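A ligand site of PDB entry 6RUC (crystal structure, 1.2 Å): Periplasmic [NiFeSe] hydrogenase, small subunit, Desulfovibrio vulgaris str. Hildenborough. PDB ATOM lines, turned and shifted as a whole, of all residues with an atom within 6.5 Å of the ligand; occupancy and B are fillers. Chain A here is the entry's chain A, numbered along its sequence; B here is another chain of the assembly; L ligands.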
ATOM      1  N   GLN A  16      10.360  20.236  12.062  1.00  0.00           N
ATOM      2  CA  GLN A  16       8.920  20.227  12.322  1.00  0.00           C
ATOM      3  C   GLN A  16       8.523  18.931  13.035  1.00  0.00           C
ATOM      4  O   GLN A  16       7.825  18.076  12.480  1.00  0.00           O
ATOM      5  CB  GLN A  16       8.155  20.385  11.029  1.00  0.00           C
ATOM      6  CG  GLN A  16       8.315  21.750  10.393  1.00  0.00           C
ATOM      7  CD  GLN A  16       7.722  21.783   9.006  1.00  0.00           C
ATOM      8  OE1 GLN A  16       8.126  20.995   8.130  1.00  0.00           O
ATOM      9  NE2 GLN A  16       6.735  22.646   8.794  1.00  0.00           N
ATOM     10  N   GLY A  17       9.052  18.782  14.253  1.00  0.00           N
ATOM     11  CA  GLY A  17       8.727  17.670  15.105  1.00  0.00           C
ATOM     12  C   GLY A  17       7.828  18.120  16.255  1.00  0.00           C
ATOM     13  O   GLY A  17       7.555  19.309  16.438  1.00  0.00           O
ATOM     14  N   CYS A  18       7.388  17.129  17.038  1.00  0.00           N
ATOM     15  CA  CYS A  18       6.522  17.375  18.184  1.00  0.00           C
ATOM     16  C   CYS A  18       7.208  17.017  19.500  1.00  0.00           C
ATOM     17  O   CYS A  18       6.572  17.107  20.552  1.00  0.00           O
ATOM     18  CB  CYS A  18       5.216  16.574  18.065  1.00  0.00           C
ATOM     19  SG  CYS A  18       5.390  14.788  18.449  1.00  0.00           S
ATOM     20  N   THR A  19       8.470  16.603  19.450  1.00  0.00           N
ATOM     21  CA  THR A  19       9.273  16.169  20.598  1.00  0.00           C
ATOM     22  C   THR A  19       8.882  14.746  21.049  1.00  0.00           C
ATOM     23  O   THR A  19       9.522  14.175  21.933  1.00  0.00           O
ATOM     24  CB  THR A  19       9.324  17.234  21.705  1.00  0.00           C
ATOM     25  OG1 THR A  19       9.809  18.446  21.099  1.00  0.00           O
ATOM     26  CG2 THR A  19      10.281  16.879  22.836  1.00  0.00           C
ATOM     27  N   GLY A  20       7.909  14.127  20.379  1.00  0.00           N
ATOM     28  CA  GLY A  20       7.523  12.768  20.731  1.00  0.00           C
ATOM     29  C   GLY A  20       8.567  11.721  20.395  1.00  0.00           C
ATOM     30  O   GLY A  20       8.604  10.671  21.047  1.00  0.00           O
ATOM     31  N   CYS A  21       9.402  11.978  19.399  1.00  0.00           N
ATOM     32  CA  CYS A  21      10.491  11.052  19.091  1.00  0.00           C
ATOM     33  C   CYS A  21      11.573  11.125  20.166  1.00  0.00           C
ATOM     34  O   CYS A  21      12.184  10.110  20.524  1.00  0.00           O
ATOM     35  CB  CYS A  21      11.020  11.317  17.685  1.00  0.00           C
ATOM     36  SG  CYS A  21       9.887  10.766  16.325  1.00  0.00           S
ATOM     37  N   SER A  22      11.806  12.319  20.721  1.00  0.00           N
ATOM     38  CA  SER A  22      12.693  12.421  21.876  1.00  0.00           C
ATOM     39  C   SER A  22      12.087  11.724  23.093  1.00  0.00           C
ATOM     40  O   SER A  22      12.775  10.996  23.808  1.00  0.00           O
ATOM     41  CB  SER A  22      12.969  13.890  22.202  1.00  0.00           C
ATOM     42  OG  SER A  22      13.831  14.515  21.262  1.00  0.00           O
ATOM     43  N   GLU A  77      14.714  14.965  13.998  1.00  0.00           N
ATOM     44  CA  GLU A  77      13.350  14.746  14.462  1.00  0.00           C
ATOM     45  C   GLU A  77      12.482  15.823  13.826  1.00  0.00           C
ATOM     46  O   GLU A  77      12.763  17.014  14.002  1.00  0.00           O
ATOM     47  CB  GLU A  77      13.304  14.828  16.002  1.00  0.00           C
ATOM     48  CG  GLU A  77      11.914  14.919  16.634  1.00  0.00           C
ATOM     49  CD  GLU A  77      11.944  14.840  18.175  1.00  0.00           C
ATOM     50  OE1 GLU A  77      12.976  15.208  18.802  1.00  0.00           O
ATOM     51  OE2 GLU A  77      10.906  14.439  18.754  1.00  0.00           O
ATOM     52  N   GLY A  78      11.453  15.428  13.095  1.00  0.00           N
ATOM     53  CA  GLY A  78      10.618  16.365  12.364  1.00  0.00           C
ATOM     54  C   GLY A  78      11.032  16.507  10.908  1.00  0.00           C
ATOM     55  O   GLY A  78      12.147  16.162  10.510  1.00  0.00           O
ATOM     56  N   SER A  79      10.119  17.050  10.093  1.00  0.00           N
ATOM     57  CA  SER A  79      10.352  17.340   8.685  1.00  0.00           C
ATOM     58  C   SER A  79      11.095  18.674   8.508  1.00  0.00           C
ATOM     59  O   SER A  79      11.276  19.450   9.455  1.00  0.00           O
ATOM     60  CB  SER A  79       9.031  17.322   7.918  1.00  0.00           C
ATOM     61  OG  SER A  79       8.095  18.221   8.483  1.00  0.00           O
ATOM     62  N   VAL A 118      14.731  10.060  12.417  1.00  0.00           N
ATOM     63  CA  VAL A 118      13.965   9.422  13.467  1.00  0.00           C
ATOM     64  C   VAL A 118      12.540   9.934  13.410  1.00  0.00           C
ATOM     65  O   VAL A 118      12.308  11.142  13.482  1.00  0.00           O
ATOM     66  CB  VAL A 118      14.604   9.663  14.850  1.00  0.00           C
ATOM     67  CG1 VAL A 118      13.743   9.116  15.947  1.00  0.00           C
ATOM     68  CG2 VAL A 118      15.964   8.983  14.918  1.00  0.00           C
ATOM     69  N   GLY A 119      11.610   9.004  13.271  1.00  0.00           N
ATOM     70  CA  GLY A 119      10.195   9.293  13.174  1.00  0.00           C
ATOM     71  C   GLY A 119       9.734   9.448  11.744  1.00  0.00           C
ATOM     72  O   GLY A 119      10.485   9.782  10.842  1.00  0.00           O
ATOM     73  N   THR A 120       8.440   9.213  11.560  1.00  0.00           N
ATOM     74  CA  THR A 120       7.834   9.328  10.234  1.00  0.00           C
ATOM     75  C   THR A 120       7.922  10.738   9.639  1.00  0.00           C
ATOM     76  O   THR A 120       8.049  10.867   8.424  1.00  0.00           O
ATOM     77  CB  THR A 120       6.410   8.790  10.333  1.00  0.00           C
ATOM     78  OG1 THR A 120       6.506   7.398  10.616  1.00  0.00           O
ATOM     79  CG2 THR A 120       5.621   9.016   9.039  1.00  0.00           C
ATOM     80  N   CYS A 121       7.859  11.799  10.458  1.00  0.00           N
ATOM     81  CA  CYS A 121       8.027  13.136   9.888  1.00  0.00           C
ATOM     82  C   CYS A 121       9.373  13.272   9.169  1.00  0.00           C
ATOM     83  O   CYS A 121       9.427  13.694   8.009  1.00  0.00           O
ATOM     84  CB  CYS A 121       7.943  14.220  10.980  1.00  0.00           C
ATOM     85  SG  CYS A 121       6.386  14.358  11.853  1.00  0.00           S
ATOM     86  N   ALA A 122      10.454  12.953   9.874  1.00  0.00           N
ATOM     87  CA  ALA A 122      11.784  13.072   9.289  1.00  0.00           C
ATOM     88  C   ALA A 122      11.982  12.059   8.161  1.00  0.00           C
ATOM     89  O   ALA A 122      12.589  12.376   7.133  1.00  0.00           O
ATOM     90  CB  ALA A 122      12.841  12.844  10.375  1.00  0.00           C
ATOM     91  N   GLY A 126       5.453  12.844   6.911  1.00  0.00           N
ATOM     92  CA  GLY A 126       4.485  12.668   7.981  1.00  0.00           C
ATOM     93  C   GLY A 126       3.380  13.706   8.007  1.00  0.00           C
ATOM     94  O   GLY A 126       2.981  14.276   6.980  1.00  0.00           O
ATOM     95  N   ILE A 127       2.856  13.937   9.211  1.00  0.00           N
ATOM     96  CA  ILE A 127       1.724  14.858   9.353  1.00  0.00           C
ATOM     97  C   ILE A 127       2.036  16.252   8.826  1.00  0.00           C
ATOM     98  O   ILE A 127       1.182  16.828   8.133  1.00  0.00           O
ATOM     99  CB  ILE A 127       1.170  14.812  10.780  1.00  0.00           C
ATOM    100  CG1 ILE A 127       0.467  13.444  11.027  1.00  0.00           C
ATOM    101  CG2 ILE A 127       0.209  15.982  11.061  1.00  0.00           C
ATOM    102  CD1 ILE A 127       0.196  13.135  12.458  1.00  0.00           C
ATOM    103  N   PRO A 128       3.213  16.843   9.054  1.00  0.00           N
ATOM    104  CA  PRO A 128       3.457  18.188   8.522  1.00  0.00           C
ATOM    105  C   PRO A 128       3.409  18.284   7.009  1.00  0.00           C
ATOM    106  O   PRO A 128       3.219  19.375   6.481  1.00  0.00           O
ATOM    107  CB  PRO A 128       4.856  18.528   9.061  1.00  0.00           C
ATOM    108  CG  PRO A 128       4.952  17.746  10.338  1.00  0.00           C
ATOM    109  CD  PRO A 128       4.279  16.430   9.993  1.00  0.00           C
ATOM    110  N   GLY A 158       7.852   5.589  12.460  1.00  0.00           N
ATOM    111  CA  GLY A 158       6.928   5.468  13.569  1.00  0.00           C
ATOM    112  C   GLY A 158       6.529   6.857  14.024  1.00  0.00           C
ATOM    113  O   GLY A 158       7.266   7.834  13.857  1.00  0.00           O
ATOM    114  N   CYS A 159       5.355   6.964  14.637  1.00  0.00           N
ATOM    115  CA  CYS A 159       4.838   8.250  15.088  1.00  0.00           C
ATOM    116  C   CYS A 159       4.225   8.039  16.463  1.00  0.00           C
ATOM    117  O   CYS A 159       3.000   7.988  16.639  1.00  0.00           O
ATOM    118  CB  CYS A 159       3.849   8.823  14.075  1.00  0.00           C
ATOM    119  SG  CYS A 159       3.410  10.544  14.348  1.00  0.00           S
ATOM    120  N   PRO A 160       5.061   7.889  17.490  1.00  0.00           N
ATOM    121  CA  PRO A 160       6.530   7.839  17.413  1.00  0.00           C
ATOM    122  C   PRO A 160       7.054   6.424  17.147  1.00  0.00           C
ATOM    123  O   PRO A 160       6.296   5.443  17.259  1.00  0.00           O
ATOM    124  CB  PRO A 160       6.938   8.230  18.833  1.00  0.00           C
ATOM    125  CG  PRO A 160       5.886   7.589  19.682  1.00  0.00           C
ATOM    126  CD  PRO A 160       4.581   7.682  18.873  1.00  0.00           C
ATOM    127  N   PRO A 161       8.338   6.292  16.816  1.00  0.00           N
ATOM    128  CA  PRO A 161       8.989   4.984  16.881  1.00  0.00           C
ATOM    129  C   PRO A 161       8.943   4.407  18.289  1.00  0.00           C
ATOM    130  O   PRO A 161       8.862   5.127  19.284  1.00  0.00           O
ATOM    131  CB  PRO A 161      10.439   5.286  16.480  1.00  0.00           C
ATOM    132  CG  PRO A 161      10.412   6.656  15.836  1.00  0.00           C
ATOM    133  CD  PRO A 161       9.295   7.383  16.524  1.00  0.00           C
ATOM    134  N   PHE A 273       1.799   7.570   5.750  1.00  0.00           N
ATOM    135  CA  PHE A 273       1.110   8.033   6.945  1.00  0.00           C
ATOM    136  C   PHE A 273       1.178   9.548   7.024  1.00  0.00           C
ATOM    137  O   PHE A 273       2.273  10.113   6.897  1.00  0.00           O
ATOM    138  CB  PHE A 273       1.750   7.408   8.188  1.00  0.00           C
ATOM    139  CG  PHE A 273       1.108   7.870   9.483  1.00  0.00           C
ATOM    140  CD1 PHE A 273      -0.021   7.232   9.984  1.00  0.00           C
ATOM    141  CD2 PHE A 273       1.659   8.918  10.221  1.00  0.00           C
ATOM    142  CE1 PHE A 273      -0.604   7.657  11.167  1.00  0.00           C
ATOM    143  CE2 PHE A 273       1.079   9.329  11.414  1.00  0.00           C
ATOM    144  CZ  PHE A 273      -0.050   8.697  11.894  1.00  0.00           C
ATOM    145  N   ARG B  50       3.655  24.361  11.807  1.00  0.00           N
ATOM    146  CA  ARG B  50       3.156  23.245  11.006  1.00  0.00           C
ATOM    147  C   ARG B  50       1.751  23.457  10.435  1.00  0.00           C
ATOM    148  O   ARG B  50       1.476  22.987   9.333  1.00  0.00           O
ATOM    149  CB  ARG B  50       3.198  21.956  11.826  1.00  0.00           C
ATOM    150  CG  ARG B  50       4.639  21.492  12.064  1.00  0.00           C
ATOM    151  CD  ARG B  50       4.812  20.500  13.201  1.00  0.00           C
ATOM    152  NE  ARG B  50       4.385  21.122  14.442  1.00  0.00           N
ATOM    153  CZ  ARG B  50       4.000  20.465  15.534  1.00  0.00           C
ATOM    154  NH1 ARG B  50       4.046  19.144  15.560  1.00  0.00           N
ATOM    155  NH2 ARG B  50       3.556  21.130  16.607  1.00  0.00           N
ATOM    156  N   PHE B  52      -1.600  22.683  11.914  1.00  0.00           N
ATOM    157  CA  PHE B  52      -2.604  21.656  12.148  1.00  0.00           C
ATOM    158  C   PHE B  52      -4.006  22.132  11.829  1.00  0.00           C
ATOM    159  O   PHE B  52      -4.845  21.340  11.385  1.00  0.00           O
ATOM    160  CB  PHE B  52      -2.503  21.161  13.582  1.00  0.00           C
ATOM    161  CG  PHE B  52      -1.388  20.168  13.801  1.00  0.00           C
ATOM    162  CD1 PHE B  52      -0.064  20.594  13.860  1.00  0.00           C
ATOM    163  CD2 PHE B  52      -1.653  18.833  13.912  1.00  0.00           C
ATOM    164  CE1 PHE B  52       0.957  19.685  14.014  1.00  0.00           C
ATOM    165  CE2 PHE B  52      -0.638  17.914  14.073  1.00  0.00           C
ATOM    166  CZ  PHE B  52       0.673  18.341  14.138  1.00  0.00           C
ATOM    167  N   ARG B  70      -0.288  14.883  17.585  1.00  0.00           N
ATOM    168  CA  ARG B  70       1.030  15.168  17.008  1.00  0.00           C
ATOM    169  C   ARG B  70       1.396  16.638  17.042  1.00  0.00           C
ATOM    170  O   ARG B  70       2.496  17.003  16.609  1.00  0.00           O
ATOM    171  CB  ARG B  70       1.177  14.562  15.616  1.00  0.00           C
ATOM    172  CG  ARG B  70       1.410  13.056  15.657  1.00  0.00           C
ATOM    173  CD  ARG B  70       0.201  12.235  15.982  1.00  0.00           C
ATOM    174  NE  ARG B  70       0.543  10.808  15.952  1.00  0.00           N
ATOM    175  CZ  ARG B  70      -0.233   9.822  16.366  1.00  0.00           C
ATOM    176  NH1 ARG B  70      -1.468  10.051  16.780  1.00  0.00           N
ATOM    177  NH2 ARG B  70       0.234   8.587  16.357  1.00  0.00           N
ATOM    178  N   ILE B  71       0.533  17.496  17.590  1.00  0.00           N
ATOM    179  CA  ILE B  71       0.949  18.831  17.973  1.00  0.00           C
ATOM    180  C   ILE B  71       2.135  18.737  18.927  1.00  0.00           C
ATOM    181  O   ILE B  71       3.056  19.544  18.844  1.00  0.00           O
ATOM    182  CB  ILE B  71      -0.211  19.623  18.595  1.00  0.00           C
ATOM    183  CG1 ILE B  71      -1.221  19.983  17.484  1.00  0.00           C
ATOM    184  CG2 ILE B  71       0.306  20.865  19.334  1.00  0.00           C
ATOM    185  CD1 ILE B  71      -2.523  20.552  17.972  1.00  0.00           C
ATOM    186  N   CSD B  72       2.108  17.755  19.827  1.00  0.00           N
ATOM    187  CA  CSD B  72       3.117  17.713  20.918  1.00  0.00           C
ATOM    188  CB  CSD B  72       2.801  18.750  21.994  1.00  0.00           C
ATOM    189  SG  CSD B  72       3.937  18.697  23.254  1.00  0.00           S
ATOM    190  C   CSD B  72       3.176  16.352  21.545  1.00  0.00           C
ATOM    191  O   CSD B  72       2.153  15.832  22.035  1.00  0.00           O
ATOM    192  N   GLY B  73       4.367  15.771  21.548  1.00  0.00           N
ATOM    193  CA  GLY B  73       4.576  14.457  22.119  1.00  0.00           C
ATOM    194  C   GLY B  73       4.919  14.447  23.605  1.00  0.00           C
ATOM    195  O   GLY B  73       5.090  13.364  24.159  1.00  0.00           O
ATOM    196  N   PRO B 181       4.373   8.094  23.818  1.00  0.00           N
ATOM    197  CA  PRO B 181       3.484   9.127  23.254  1.00  0.00           C
ATOM    198  C   PRO B 181       2.432   8.621  22.262  1.00  0.00           C
ATOM    199  O   PRO B 181       2.625   7.590  21.608  1.00  0.00           O
ATOM    200  CB  PRO B 181       4.450  10.088  22.535  1.00  0.00           C
ATOM    201  CG  PRO B 181       5.755   9.906  23.231  1.00  0.00           C
ATOM    202  CD  PRO B 181       5.793   8.443  23.599  1.00  0.00           C
ATOM    203  N   HIS B 182       1.337   9.383  22.208  1.00  0.00           N
ATOM    204  CA  HIS B 182       0.289   9.297  21.202  1.00  0.00           C
ATOM    205  C   HIS B 182      -0.620   8.099  21.467  1.00  0.00           C
ATOM    206  O   HIS B 182      -0.505   7.020  20.859  1.00  0.00           O
ATOM    207  CB  HIS B 182       0.854   9.350  19.781  1.00  0.00           C
ATOM    208  CG  HIS B 182       1.647  10.589  19.524  1.00  0.00           C
ATOM    209  ND1 HIS B 182       1.399  11.776  20.175  1.00  0.00           N
ATOM    210  CD2 HIS B 182       2.712  10.812  18.708  1.00  0.00           C
ATOM    211  CE1 HIS B 182       2.262  12.682  19.768  1.00  0.00           C
ATOM    212  NE2 HIS B 182       3.064  12.126  18.879  1.00  0.00           N
HETATM  213 FE1  LIG L   1       6.111  13.740  16.570  1.00  0.00          FE
HETATM  214 FE2  LIG L   1       6.775  13.495  13.947  1.00  0.00          FE
HETATM  215 FE3  LIG L   1       5.286  11.637  15.123  1.00  0.00          FE
HETATM  216 FE4  LIG L   1       7.953  11.858  15.904  1.00  0.00          FE
HETATM  217  S1  LIG L   1       7.174  11.220  13.839  1.00  0.00           S
HETATM  218  S2  LIG L   1       6.083  11.517  17.239  1.00  0.00           S
HETATM  219  S3  LIG L   1       8.207  14.168  15.610  1.00  0.00           S
HETATM  220  S4  LIG L   1       4.688  13.855  14.839  1.00  0.00           S
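An iron atom (FE4) of the ligand is bound by the side-chain sulfur of Cys 21.
The backbone NH (N) of Cys 18 sits close to a sulfur (S3) of the ligand (3.4 Å).
An iron atom (FE1) of the ligand is bound by the side-chain sulfur of Cys 18 (2.3 Å).
The backbone NH (N) of Cys 121 sits close to a sulfur (S1) of the ligand, at 3.5 Å.
SG of Cys 121 binds FE2 of the ligand.
SG of Cys 159 binds FE3 of the ligand.
The backbone NH of Thr 120 sits close to a sulfur (S1) of the ligand, at 3.3 Å.
A ring nitrogen (NE2) of His 182 of chain B lies close to a sulfur (S2) of the ligand (3.5 Å).
SG of Cys 21 sits close to O of Val 118, at 3.8 Å.
SG of Cys 18 sits close to N of Gly 20, 3.2 Å away.
The backbone NH of Gly 73 of chain B lies within hydrogen-bond range of the backbone carbonyl oxygen of Cys 18.
OG1 of Thr 120 lies within hydrogen-bond range of N of Gly 158, 2.9 Å away.
The backbone carbonyl oxygen (O) of Arg 70 of chain B is in hydrogen-bond range of the guanidinium group (NH1) of Arg 50 of chain B.
The backbone NH of Gly 20 sits at hydrogen-bond distance from the side-chain carboxylate of Glu 77.
The backbone NH (N) of Thr 19 sits close to the side-chain carboxylate (OE2) of Glu 77, 3.3 Å away.
OE1 of Glu 77 sits at hydrogen-bond distance from OG of Ser 22, 2.7 Å away.
S1 of the ligand lies close to O of Gly 158 (3.4 Å).
S2 of the ligand sits close to N of Pro 160, 3.8 Å away.
CA of Gly 17 touches S3 of the ligand, 3.6 Å away.
Gly 20 touches the ligand.
Glu 77 touches the ligand.
Gly 119 touches the ligand (CA to S1, 3.6 Å).
CG of Arg 70 of chain B touches S4 of the ligand, at 3.5 Å.
Hydrophobic or aromatic side chains that line the ligand: Pro 160 and His 182 of chain B.
Within 4 Å of the ligand: Gly 17, Cys 18, Gly 20, Cys 21, Glu 77, Gly 119, Thr 120, Cys 121, Gly 158, Cys 159, Pro 160, Arg 70 of chain B and His 182 of chain B.
The nearest printed residue that does not touch the ligand is Gly 78 (4.3 Å).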
